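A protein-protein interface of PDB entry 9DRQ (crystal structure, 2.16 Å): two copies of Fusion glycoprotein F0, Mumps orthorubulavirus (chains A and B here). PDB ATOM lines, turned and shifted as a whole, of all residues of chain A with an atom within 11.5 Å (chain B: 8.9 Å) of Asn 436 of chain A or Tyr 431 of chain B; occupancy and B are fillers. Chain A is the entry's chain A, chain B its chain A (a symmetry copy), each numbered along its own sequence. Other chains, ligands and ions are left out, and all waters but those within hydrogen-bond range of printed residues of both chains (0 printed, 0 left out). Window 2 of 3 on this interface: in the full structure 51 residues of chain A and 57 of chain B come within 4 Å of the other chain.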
ATOM      1  N   LEU A 425     -16.544  18.847   0.267  1.00  0.00           N
ATOM      2  CA  LEU A 425     -16.571  19.272   1.660  1.00  0.00           C
ATOM      3  C   LEU A 425     -17.900  18.922   2.308  1.00  0.00           C
ATOM      4  O   LEU A 425     -17.937  18.329   3.390  1.00  0.00           O
ATOM      5  CB  LEU A 425     -16.315  20.770   1.765  1.00  0.00           C
ATOM      6  CG  LEU A 425     -16.515  21.393   3.150  1.00  0.00           C
ATOM      7  CD1 LEU A 425     -15.605  20.718   4.200  1.00  0.00           C
ATOM      8  CD2 LEU A 425     -16.304  22.917   3.130  1.00  0.00           C
ATOM      9  N   ASN A 427     -20.130  16.798   1.545  1.00  0.00           N
ATOM     10  CA  ASN A 427     -20.282  15.365   1.715  1.00  0.00           C
ATOM     11  C   ASN A 427     -19.443  14.869   2.880  1.00  0.00           C
ATOM     12  O   ASN A 427     -19.879  13.998   3.642  1.00  0.00           O
ATOM     13  CB  ASN A 427     -19.909  14.657   0.425  1.00  0.00           C
ATOM     14  CG  ASN A 427     -20.356  13.235   0.414  1.00  0.00           C
ATOM     15  OD1 ASN A 427     -21.557  12.951   0.453  1.00  0.00           O
ATOM     16  ND2 ASN A 427     -19.405  12.321   0.363  1.00  0.00           N
ATOM     17  N   ALA A 428     -18.245  15.437   3.054  1.00  0.00           N
ATOM     18  CA  ALA A 428     -17.394  15.030   4.165  1.00  0.00           C
ATOM     19  C   ALA A 428     -17.992  15.462   5.501  1.00  0.00           C
ATOM     20  O   ALA A 428     -17.967  14.695   6.475  1.00  0.00           O
ATOM     21  CB  ALA A 428     -15.984  15.590   3.982  1.00  0.00           C
ATOM     22  N   VAL A 429     -18.549  16.677   5.566  1.00  0.00           N
ATOM     23  CA  VAL A 429     -19.220  17.115   6.792  1.00  0.00           C
ATOM     24  C   VAL A 429     -20.297  16.106   7.195  1.00  0.00           C
ATOM     25  O   VAL A 429     -20.372  15.672   8.351  1.00  0.00           O
ATOM     26  CB  VAL A 429     -19.794  18.535   6.619  1.00  0.00           C
ATOM     27  CG1 VAL A 429     -20.533  18.960   7.874  1.00  0.00           C
ATOM     28  CG2 VAL A 429     -18.685  19.540   6.295  1.00  0.00           C
ATOM     29  N   LYS A 430     -21.128  15.699   6.233  1.00  0.00           N
ATOM     30  CA  LYS A 430     -22.133  14.673   6.494  1.00  0.00           C
ATOM     31  C   LYS A 430     -21.489  13.387   6.987  1.00  0.00           C
ATOM     32  O   LYS A 430     -21.989  12.751   7.922  1.00  0.00           O
ATOM     33  CB  LYS A 430     -22.951  14.419   5.227  1.00  0.00           C
ATOM     34  CG  LYS A 430     -23.920  13.258   5.313  1.00  0.00           C
ATOM     35  CD  LYS A 430     -24.268  12.739   3.926  1.00  0.00           C
ATOM     36  CE  LYS A 430     -25.030  13.768   3.125  1.00  0.00           C
ATOM     37  NZ  LYS A 430     -26.484  13.730   3.458  1.00  0.00           N
ATOM     38  N   TYR A 431     -20.376  12.983   6.377  1.00  0.00           N
ATOM     39  CA  TYR A 431     -19.671  11.800   6.862  1.00  0.00           C
ATOM     40  C   TYR A 431     -19.246  11.971   8.317  1.00  0.00           C
ATOM     41  O   TYR A 431     -19.269  11.006   9.092  1.00  0.00           O
ATOM     42  CB  TYR A 431     -18.457  11.528   5.975  1.00  0.00           C
ATOM     43  CG  TYR A 431     -18.016  10.080   5.878  1.00  0.00           C
ATOM     44  CD1 TYR A 431     -17.623   9.363   7.007  1.00  0.00           C
ATOM     45  CD2 TYR A 431     -17.951   9.442   4.640  1.00  0.00           C
ATOM     46  CE1 TYR A 431     -17.201   8.042   6.907  1.00  0.00           C
ATOM     47  CE2 TYR A 431     -17.529   8.127   4.531  1.00  0.00           C
ATOM     48  CZ  TYR A 431     -17.156   7.431   5.665  1.00  0.00           C
ATOM     49  OH  TYR A 431     -16.739   6.125   5.555  1.00  0.00           O
ATOM     50  N   ILE A 432     -18.897  13.199   8.714  1.00  0.00           N
ATOM     51  CA  ILE A 432     -18.392  13.441  10.064  1.00  0.00           C
ATOM     52  C   ILE A 432     -19.513  13.350  11.088  1.00  0.00           C
ATOM     53  O   ILE A 432     -19.334  12.782  12.175  1.00  0.00           O
ATOM     54  CB  ILE A 432     -17.683  14.806  10.128  1.00  0.00           C
ATOM     55  CG1 ILE A 432     -16.424  14.763   9.277  1.00  0.00           C
ATOM     56  CG2 ILE A 432     -17.337  15.172  11.561  1.00  0.00           C
ATOM     57  CD1 ILE A 432     -15.834  13.368   9.197  1.00  0.00           C
ATOM     58  N   LYS A 433     -20.673  13.934  10.776  1.00  0.00           N
ATOM     59  CA  LYS A 433     -21.817  13.836  11.675  1.00  0.00           C
ATOM     60  C   LYS A 433     -22.231  12.383  11.852  1.00  0.00           C
ATOM     61  O   LYS A 433     -22.403  11.907  12.980  1.00  0.00           O
ATOM     62  CB  LYS A 433     -22.982  14.679  11.148  1.00  0.00           C
ATOM     63  CG  LYS A 433     -22.620  16.146  10.835  1.00  0.00           C
ATOM     64  CD  LYS A 433     -22.016  16.852  12.047  1.00  0.00           C
ATOM     65  CE  LYS A 433     -21.611  18.283  11.713  1.00  0.00           C
ATOM     66  NZ  LYS A 433     -20.837  18.937  12.812  1.00  0.00           N
ATOM     67  N   GLU A 434     -22.362  11.652  10.742  1.00  0.00           N
ATOM     68  CA  GLU A 434     -22.687  10.231  10.831  1.00  0.00           C
ATOM     69  C   GLU A 434     -21.567   9.455  11.508  1.00  0.00           C
ATOM     70  O   GLU A 434     -21.827   8.544  12.303  1.00  0.00           O
ATOM     71  CB  GLU A 434     -22.991   9.673   9.437  1.00  0.00           C
ATOM     72  CG  GLU A 434     -24.030  10.506   8.675  1.00  0.00           C
ATOM     73  CD  GLU A 434     -24.598   9.812   7.450  1.00  0.00           C
ATOM     74  OE1 GLU A 434     -25.010  10.527   6.501  1.00  0.00           O
ATOM     75  OE2 GLU A 434     -24.645   8.556   7.446  1.00  0.00           O
ATOM     76  N   SER A 435     -20.312   9.807  11.222  1.00  0.00           N
ATOM     77  CA  SER A 435     -19.196   9.219  11.955  1.00  0.00           C
ATOM     78  C   SER A 435     -19.304   9.531  13.444  1.00  0.00           C
ATOM     79  O   SER A 435     -19.213   8.632  14.286  1.00  0.00           O
ATOM     80  CB  SER A 435     -17.866   9.726  11.394  1.00  0.00           C
ATOM     81  OG  SER A 435     -16.827   8.777  11.555  1.00  0.00           O
ATOM     82  N   ASN A 436     -19.520  10.806  13.787  1.00  0.00           N
ATOM     83  CA  ASN A 436     -19.626  11.174  15.194  1.00  0.00           C
ATOM     84  C   ASN A 436     -20.865  10.570  15.845  1.00  0.00           C
ATOM     85  O   ASN A 436     -20.847  10.273  17.046  1.00  0.00           O
ATOM     86  CB  ASN A 436     -19.634  12.692  15.346  1.00  0.00           C
ATOM     87  CG  ASN A 436     -19.634  13.127  16.792  1.00  0.00           C
ATOM     88  OD1 ASN A 436     -20.678  13.163  17.436  1.00  0.00           O
ATOM     89  ND2 ASN A 436     -18.459  13.462  17.311  1.00  0.00           N
ATOM     90  N   HIS A 437     -21.945  10.376  15.080  1.00  0.00           N
ATOM     91  CA  HIS A 437     -23.123   9.711  15.630  1.00  0.00           C
ATOM     92  C   HIS A 437     -22.823   8.250  15.949  1.00  0.00           C
ATOM     93  O   HIS A 437     -22.951   7.815  17.100  1.00  0.00           O
ATOM     94  CB  HIS A 437     -24.308   9.820  14.665  1.00  0.00           C
ATOM     95  CG  HIS A 437     -25.594   9.274  15.218  1.00  0.00           C
ATOM     96  ND1 HIS A 437     -25.668   8.591  16.414  1.00  0.00           N
ATOM     97  CD2 HIS A 437     -26.860   9.325  14.740  1.00  0.00           C
ATOM     98  CE1 HIS A 437     -26.919   8.240  16.645  1.00  0.00           C
ATOM     99  NE2 HIS A 437     -27.663   8.674  15.643  1.00  0.00           N
ATOM    100  N   GLN A 438     -22.390   7.474  14.946  1.00  0.00           N
ATOM    101  CA  GLN A 438     -22.151   6.059  15.237  1.00  0.00           C
ATOM    102  C   GLN A 438     -20.974   5.859  16.190  1.00  0.00           C
ATOM    103  O   GLN A 438     -20.468   4.746  16.338  1.00  0.00           O
ATOM    104  CB  GLN A 438     -21.945   5.254  13.946  1.00  0.00           C
ATOM    105  CG  GLN A 438     -20.562   5.315  13.306  1.00  0.00           C
ATOM    106  CD  GLN A 438     -20.383   4.245  12.228  1.00  0.00           C
ATOM    107  OE1 GLN A 438     -21.241   3.380  12.050  1.00  0.00           O
ATOM    108  NE2 GLN A 438     -19.264   4.305  11.506  1.00  0.00           N
ATOM    109  N   LEU A 439     -20.554   6.930  16.860  1.00  0.00           N
ATOM    110  CA  LEU A 439     -19.617   6.852  17.969  1.00  0.00           C
ATOM    111  C   LEU A 439     -20.316   6.787  19.318  1.00  0.00           C
ATOM    112  O   LEU A 439     -19.640   6.772  20.350  1.00  0.00           O
ATOM    113  CB  LEU A 439     -18.665   8.048  17.940  1.00  0.00           C
ATOM    114  CG  LEU A 439     -17.314   7.885  18.643  1.00  0.00           C
ATOM    115  CD1 LEU A 439     -16.168   7.990  17.644  1.00  0.00           C
ATOM    116  CD2 LEU A 439     -17.160   8.908  19.765  1.00  0.00           C
ATOM    117  N   GLN A 440     -21.648   6.750  19.347  1.00  0.00           N
ATOM    118  CA  GLN A 440     -22.342   6.527  20.610  1.00  0.00           C
ATOM    119  C   GLN A 440     -22.165   5.086  21.058  1.00  0.00           C
ATOM    120  O   GLN A 440     -23.129   4.318  21.109  1.00  0.00           O
ATOM    121  CB  GLN A 440     -23.828   6.870  20.499  1.00  0.00           C
ATOM    122  CG  GLN A 440     -24.126   8.355  20.455  1.00  0.00           C
ATOM    123  CD  GLN A 440     -23.575   9.112  21.653  1.00  0.00           C
ATOM    124  OE1 GLN A 440     -22.369   9.350  21.760  1.00  0.00           O
ATOM    125  NE2 GLN A 440     -24.462   9.510  22.556  1.00  0.00           N
ATOM    126  N   SER A 441     -20.933   4.712  21.369  1.00  0.00           N
ATOM    127  CA  SER A 441     -20.642   3.390  21.890  1.00  0.00           C
ATOM    128  C   SER A 441     -19.532   3.542  22.919  1.00  0.00           C
ATOM    129  O   SER A 441     -18.661   4.403  22.763  1.00  0.00           O
ATOM    130  CB  SER A 441     -20.228   2.433  20.767  1.00  0.00           C
ATOM    131  OG  SER A 441     -20.944   2.684  19.566  1.00  0.00           O
ATOM    132  N   SER B 424     -15.511  26.531   6.744  1.00  0.00           N
ATOM    133  CA  SER B 424     -16.174  25.258   7.012  1.00  0.00           C
ATOM    134  C   SER B 424     -15.160  24.125   7.061  1.00  0.00           C
ATOM    135  O   SER B 424     -15.190  23.288   7.968  1.00  0.00           O
ATOM    136  CB  SER B 424     -17.235  24.979   5.949  1.00  0.00           C
ATOM    137  OG  SER B 424     -18.472  25.547   6.313  1.00  0.00           O
ATOM    138  N   LEU B 425     -14.244  24.092   6.088  1.00  0.00           N
ATOM    139  CA  LEU B 425     -13.178  23.100   6.101  1.00  0.00           C
ATOM    140  C   LEU B 425     -12.406  23.149   7.408  1.00  0.00           C
ATOM    141  O   LEU B 425     -12.194  22.119   8.054  1.00  0.00           O
ATOM    142  CB  LEU B 425     -12.234  23.318   4.925  1.00  0.00           C
ATOM    143  CG  LEU B 425     -10.954  22.477   4.924  1.00  0.00           C
ATOM    144  CD1 LEU B 425     -11.280  20.967   4.950  1.00  0.00           C
ATOM    145  CD2 LEU B 425     -10.038  22.827   3.739  1.00  0.00           C
ATOM    146  N   GLN B 426     -11.970  24.346   7.814  1.00  0.00           N
ATOM    147  CA  GLN B 426     -11.111  24.426   8.993  1.00  0.00           C
ATOM    148  C   GLN B 426     -11.868  24.012  10.236  1.00  0.00           C
ATOM    149  O   GLN B 426     -11.283  23.427  11.160  1.00  0.00           O
ATOM    150  CB  GLN B 426     -10.540  25.838   9.170  1.00  0.00           C
ATOM    151  CG  GLN B 426      -9.783  26.391   7.947  1.00  0.00           C
ATOM    152  CD  GLN B 426      -8.529  25.596   7.591  1.00  0.00           C
ATOM    153  OE1 GLN B 426      -7.788  25.181   8.472  1.00  0.00           O
ATOM    154  NE2 GLN B 426      -8.283  25.394   6.290  1.00  0.00           N
ATOM    155  N   ASN B 427     -13.166  24.288  10.270  1.00  0.00           N
ATOM    156  CA  ASN B 427     -13.966  23.812  11.383  1.00  0.00           C
ATOM    157  C   ASN B 427     -14.074  22.297  11.361  1.00  0.00           C
ATOM    158  O   ASN B 427     -14.030  21.649  12.414  1.00  0.00           O
ATOM    159  CB  ASN B 427     -15.338  24.463  11.339  1.00  0.00           C
ATOM    160  CG  ASN B 427     -16.084  24.289  12.617  1.00  0.00           C
ATOM    161  OD1 ASN B 427     -15.666  24.786  13.667  1.00  0.00           O
ATOM    162  ND2 ASN B 427     -17.198  23.581  12.553  1.00  0.00           N
ATOM    163  N   ALA B 428     -14.183  21.711  10.165  1.00  0.00           N
ATOM    164  CA  ALA B 428     -14.266  20.259  10.062  1.00  0.00           C
ATOM    165  C   ALA B 428     -12.946  19.606  10.462  1.00  0.00           C
ATOM    166  O   ALA B 428     -12.941  18.582  11.162  1.00  0.00           O
ATOM    167  CB  ALA B 428     -14.680  19.853   8.650  1.00  0.00           C
ATOM    168  N   VAL B 429     -11.816  20.188  10.046  1.00  0.00           N
ATOM    169  CA  VAL B 429     -10.516  19.662  10.471  1.00  0.00           C
ATOM    170  C   VAL B 429     -10.447  19.591  11.998  1.00  0.00           C
ATOM    171  O   VAL B 429     -10.069  18.567  12.578  1.00  0.00           O
ATOM    172  CB  VAL B 429      -9.369  20.506   9.880  1.00  0.00           C
ATOM    173  CG1 VAL B 429      -8.030  19.986  10.367  1.00  0.00           C
ATOM    174  CG2 VAL B 429      -9.413  20.494   8.349  1.00  0.00           C
ATOM    175  N   LYS B 430     -10.843  20.676  12.667  1.00  0.00           N
ATOM    176  CA  LYS B 430     -10.900  20.678  14.125  1.00  0.00           C
ATOM    177  C   LYS B 430     -11.816  19.579  14.642  1.00  0.00           C
ATOM    178  O   LYS B 430     -11.485  18.891  15.614  1.00  0.00           O
ATOM    179  CB  LYS B 430     -11.366  22.049  14.621  1.00  0.00           C
ATOM    180  CG  LYS B 430     -11.628  22.136  16.110  1.00  0.00           C
ATOM    181  CD  LYS B 430     -12.569  23.288  16.428  1.00  0.00           C
ATOM    182  CE  LYS B 430     -11.939  24.623  16.108  1.00  0.00           C
ATOM    183  NZ  LYS B 430     -11.069  25.081  17.229  1.00  0.00           N
ATOM    184  N   TYR B 431     -12.970  19.391  14.005  1.00  0.00           N
ATOM    185  CA  TYR B 431     -13.849  18.297  14.407  1.00  0.00           C
ATOM    186  C   TYR B 431     -13.143  16.951  14.284  1.00  0.00           C
ATOM    187  O   TYR B 431     -13.359  16.055  15.110  1.00  0.00           O
ATOM    188  CB  TYR B 431     -15.116  18.320  13.554  1.00  0.00           C
ATOM    189  CG  TYR B 431     -16.365  17.755  14.203  1.00  0.00           C
ATOM    190  CD1 TYR B 431     -16.423  16.432  14.639  1.00  0.00           C
ATOM    191  CD2 TYR B 431     -17.509  18.541  14.340  1.00  0.00           C
ATOM    192  CE1 TYR B 431     -17.578  15.917  15.216  1.00  0.00           C
ATOM    193  CE2 TYR B 431     -18.665  18.035  14.911  1.00  0.00           C
ATOM    194  CZ  TYR B 431     -18.696  16.724  15.347  1.00  0.00           C
ATOM    195  OH  TYR B 431     -19.845  16.223  15.915  1.00  0.00           O
ATOM    196  N   ILE B 432     -12.266  16.806  13.285  1.00  0.00           N
ATOM    197  CA  ILE B 432     -11.609  15.525  13.036  1.00  0.00           C
ATOM    198  C   ILE B 432     -10.557  15.238  14.097  1.00  0.00           C
ATOM    199  O   ILE B 432     -10.432  14.101  14.574  1.00  0.00           O
ATOM    200  CB  ILE B 432     -10.999  15.507  11.623  1.00  0.00           C
ATOM    201  CG1 ILE B 432     -12.115  15.544  10.590  1.00  0.00           C
ATOM    202  CG2 ILE B 432     -10.134  14.275  11.419  1.00  0.00           C
ATOM    203  CD1 ILE B 432     -13.390  14.905  11.101  1.00  0.00           C
ATOM    204  N   LYS B 433      -9.764  16.250  14.458  1.00  0.00           N
ATOM    205  CA  LYS B 433      -8.774  16.075  15.516  1.00  0.00           C
ATOM    206  C   LYS B 433      -9.456  15.721  16.828  1.00  0.00           C
ATOM    207  O   LYS B 433      -9.074  14.756  17.500  1.00  0.00           O
ATOM    208  CB  LYS B 433      -7.922  17.339  15.662  1.00  0.00           C
ATOM    209  CG  LYS B 433      -7.280  17.832  14.348  1.00  0.00           C
ATOM    210  CD  LYS B 433      -6.434  16.747  13.687  1.00  0.00           C
ATOM    211  CE  LYS B 433      -5.849  17.226  12.363  1.00  0.00           C
ATOM    212  NZ  LYS B 433      -5.183  16.130  11.595  1.00  0.00           N
ATOM    213  N   GLU B 434     -10.496  16.477  17.192  1.00  0.00           N
ATOM    214  CA  GLU B 434     -11.248  16.159  18.402  1.00  0.00           C
ATOM    215  C   GLU B 434     -11.952  14.815  18.274  1.00  0.00           C
ATOM    216  O   GLU B 434     -12.002  14.040  19.235  1.00  0.00           O
ATOM    217  CB  GLU B 434     -12.242  17.282  18.714  1.00  0.00           C
ATOM    218  CG  GLU B 434     -11.587  18.670  18.731  1.00  0.00           C
ATOM    219  CD  GLU B 434     -12.450  19.751  19.356  1.00  0.00           C
ATOM    220  OE1 GLU B 434     -12.286  20.937  18.972  1.00  0.00           O
ATOM    221  OE2 GLU B 434     -13.279  19.415  20.240  1.00  0.00           O
ATOM    222  N   SER B 435     -12.485  14.511  17.090  1.00  0.00           N
ATOM    223  CA  SER B 435     -13.029  13.179  16.847  1.00  0.00           C
ATOM    224  C   SER B 435     -11.947  12.118  17.013  1.00  0.00           C
ATOM    225  O   SER B 435     -12.138  11.127  17.728  1.00  0.00           O
ATOM    226  CB  SER B 435     -13.648  13.104  15.450  1.00  0.00           C
ATOM    227  OG  SER B 435     -14.712  12.170  15.391  1.00  0.00           O
ATOM    228  N   ASN B 436     -10.791  12.317  16.370  1.00  0.00           N
ATOM    229  CA  ASN B 436      -9.718  11.337  16.481  1.00  0.00           C
ATOM    230  C   ASN B 436      -9.159  11.265  17.897  1.00  0.00           C
ATOM    231  O   ASN B 436      -8.709  10.195  18.327  1.00  0.00           O
ATOM    232  CB  ASN B 436      -8.604  11.657  15.488  1.00  0.00           C
ATOM    233  CG  ASN B 436      -7.515  10.611  15.484  1.00  0.00           C
ATOM    234  OD1 ASN B 436      -6.625  10.630  16.328  1.00  0.00           O
ATOM    235  ND2 ASN B 436      -7.580   9.688  14.531  1.00  0.00           N
ATOM    236  N   HIS B 437      -9.180  12.377  18.637  1.00  0.00           N
ATOM    237  CA  HIS B 437      -8.749  12.339  20.033  1.00  0.00           C
ATOM    238  C   HIS B 437      -9.708  11.505  20.875  1.00  0.00           C
ATOM    239  O   HIS B 437      -9.308  10.512  21.492  1.00  0.00           O
ATOM    240  CB  HIS B 437      -8.623  13.756  20.602  1.00  0.00           C
ATOM    241  CG  HIS B 437      -8.057  13.803  21.992  1.00  0.00           C
ATOM    242  ND1 HIS B 437      -7.825  12.674  22.749  1.00  0.00           N
ATOM    243  CD2 HIS B 437      -7.664  14.850  22.756  1.00  0.00           C
ATOM    244  CE1 HIS B 437      -7.322  13.022  23.918  1.00  0.00           C
ATOM    245  NE2 HIS B 437      -7.213  14.338  23.948  1.00  0.00           N
ATOM    246  N   GLN B 438     -10.998  11.874  20.892  1.00  0.00           N
ATOM    247  CA  GLN B 438     -11.912  11.107  21.740  1.00  0.00           C
ATOM    248  C   GLN B 438     -12.101   9.677  21.236  1.00  0.00           C
ATOM    249  O   GLN B 438     -13.020   8.978  21.663  1.00  0.00           O
ATOM    250  CB  GLN B 438     -13.266  11.816  21.880  1.00  0.00           C
ATOM    251  CG  GLN B 438     -14.255  11.649  20.732  1.00  0.00           C
ATOM    252  CD  GLN B 438     -15.659  12.123  21.113  1.00  0.00           C
ATOM    253  OE1 GLN B 438     -15.920  12.452  22.270  1.00  0.00           O
ATOM    254  NE2 GLN B 438     -16.564  12.156  20.135  1.00  0.00           N
ATOM    255  N   LEU B 439     -11.214   9.230  20.348  1.00  0.00           N
ATOM    256  CA  LEU B 439     -11.119   7.832  19.963  1.00  0.00           C
ATOM    257  C   LEU B 439     -10.078   7.074  20.773  1.00  0.00           C
ATOM    258  O   LEU B 439      -9.853   5.889  20.514  1.00  0.00           O
ATOM    259  CB  LEU B 439     -10.793   7.716  18.474  1.00  0.00           C
ATOM    260  CG  LEU B 439     -11.181   6.412  17.771  1.00  0.00           C
ATOM    261  CD1 LEU B 439     -12.222   6.670  16.687  1.00  0.00           C
ATOM    262  CD2 LEU B 439      -9.949   5.720  17.194  1.00  0.00           C
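The side-chain amide nitrogen of Asn 436 of chain A lies close to the side-chain hydroxyl of Tyr 431 of chain B (3.4 Å).
Leu 425 of chain A touches Ser 424 of chain B (CD2 to CB, 3.6 Å).
Leu 425 of chain B touches Leu 425 of chain A (N to CD2, 3.8 Å).
Ile 432 of chain A touches Tyr 431 of chain B (CG2 to CD1, 3.4 Å).
Ile 432 of chain A touches Ile 432 of chain B.
Tyr 431 of chain B touches Lys 433 of chain A.
NE2 of Gln 438 of chain B touches ND2 of Asn 436 of chain A, at 3.6 Å.
Gln 438 of chain B touches Leu 439 of chain A (NE2 to CD2, 3.3 Å).
Of the printed residues of chain B, Ile 432 of chain A touches Tyr 431 (3.4 Å) and Ile 432 (3.5 Å).
Printed residues of chain B within 4 Å of Lys 433 of chain A: Tyr 431 (3.2 Å).
No residue of chain B comes within 4 Å of Ser 435 of chain A.
Of chain B, only Tyr 431 and Gln 438 come within 4 Å of Asn 436 of chain A.
Of the printed residues of chain A, Ser 424 of chain B touches Leu 425.
No residue of chain A comes within 4 Å of Val 429 of chain B.
No residue of chain A comes within 4 Å of Lys 430 of chain B.
Tyr 431 of chain B touches just these residues of chain A: Ile 432 (3.4 Å), Lys 433 (3.2 Å) and Asn 436 (3.2 Å).
Glu 434 of chain B touches none of the printed residues of chain A.
The nearest residue of chain B that does not touch Asn 436 of chain A is Ser 435 of chain B (4.4 Å).
The nearest residue of chain A that does not touch Tyr 431 of chain B is His 437 of chain A (6.3 Å).
Of the 16 printed residues of chain B, 5 touch a printed residue of chain A.
Along chain B the printed residues that touch a printed residue of chain A span positions 424 to 438.
Printed residues of chain A that touch a printed residue of chain B: Leu 425, Ile 432, Lys 433, Asn 436 and Leu 439.
Hydrophobic or aromatic side chains of chain A that line the printed part of chain B: Leu 425, Ile 432 and Leu 439.
Among the printed residues, 8 pairs touch across the chains.
Leu 425 of chain B touches its own counterpart, Leu 425 of chain A.
Ile 432 of chain A touches Tyr 431 of chain B, but with the chains exchanged Tyr 431 of chain A does not touch Ile 432 of chain B (7.1 Å).
Asn 436 of chain A touches Gln 438 of chain B, but with the chains exchanged Gln 438 of chain A does not touch Asn 436 of chain B (12.1 Å).
Leu 439 of chain A touches Gln 438 of chain B, but with the chains exchanged Gln 438 of chain A does not touch Leu 439 of chain B (8.5 Å).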
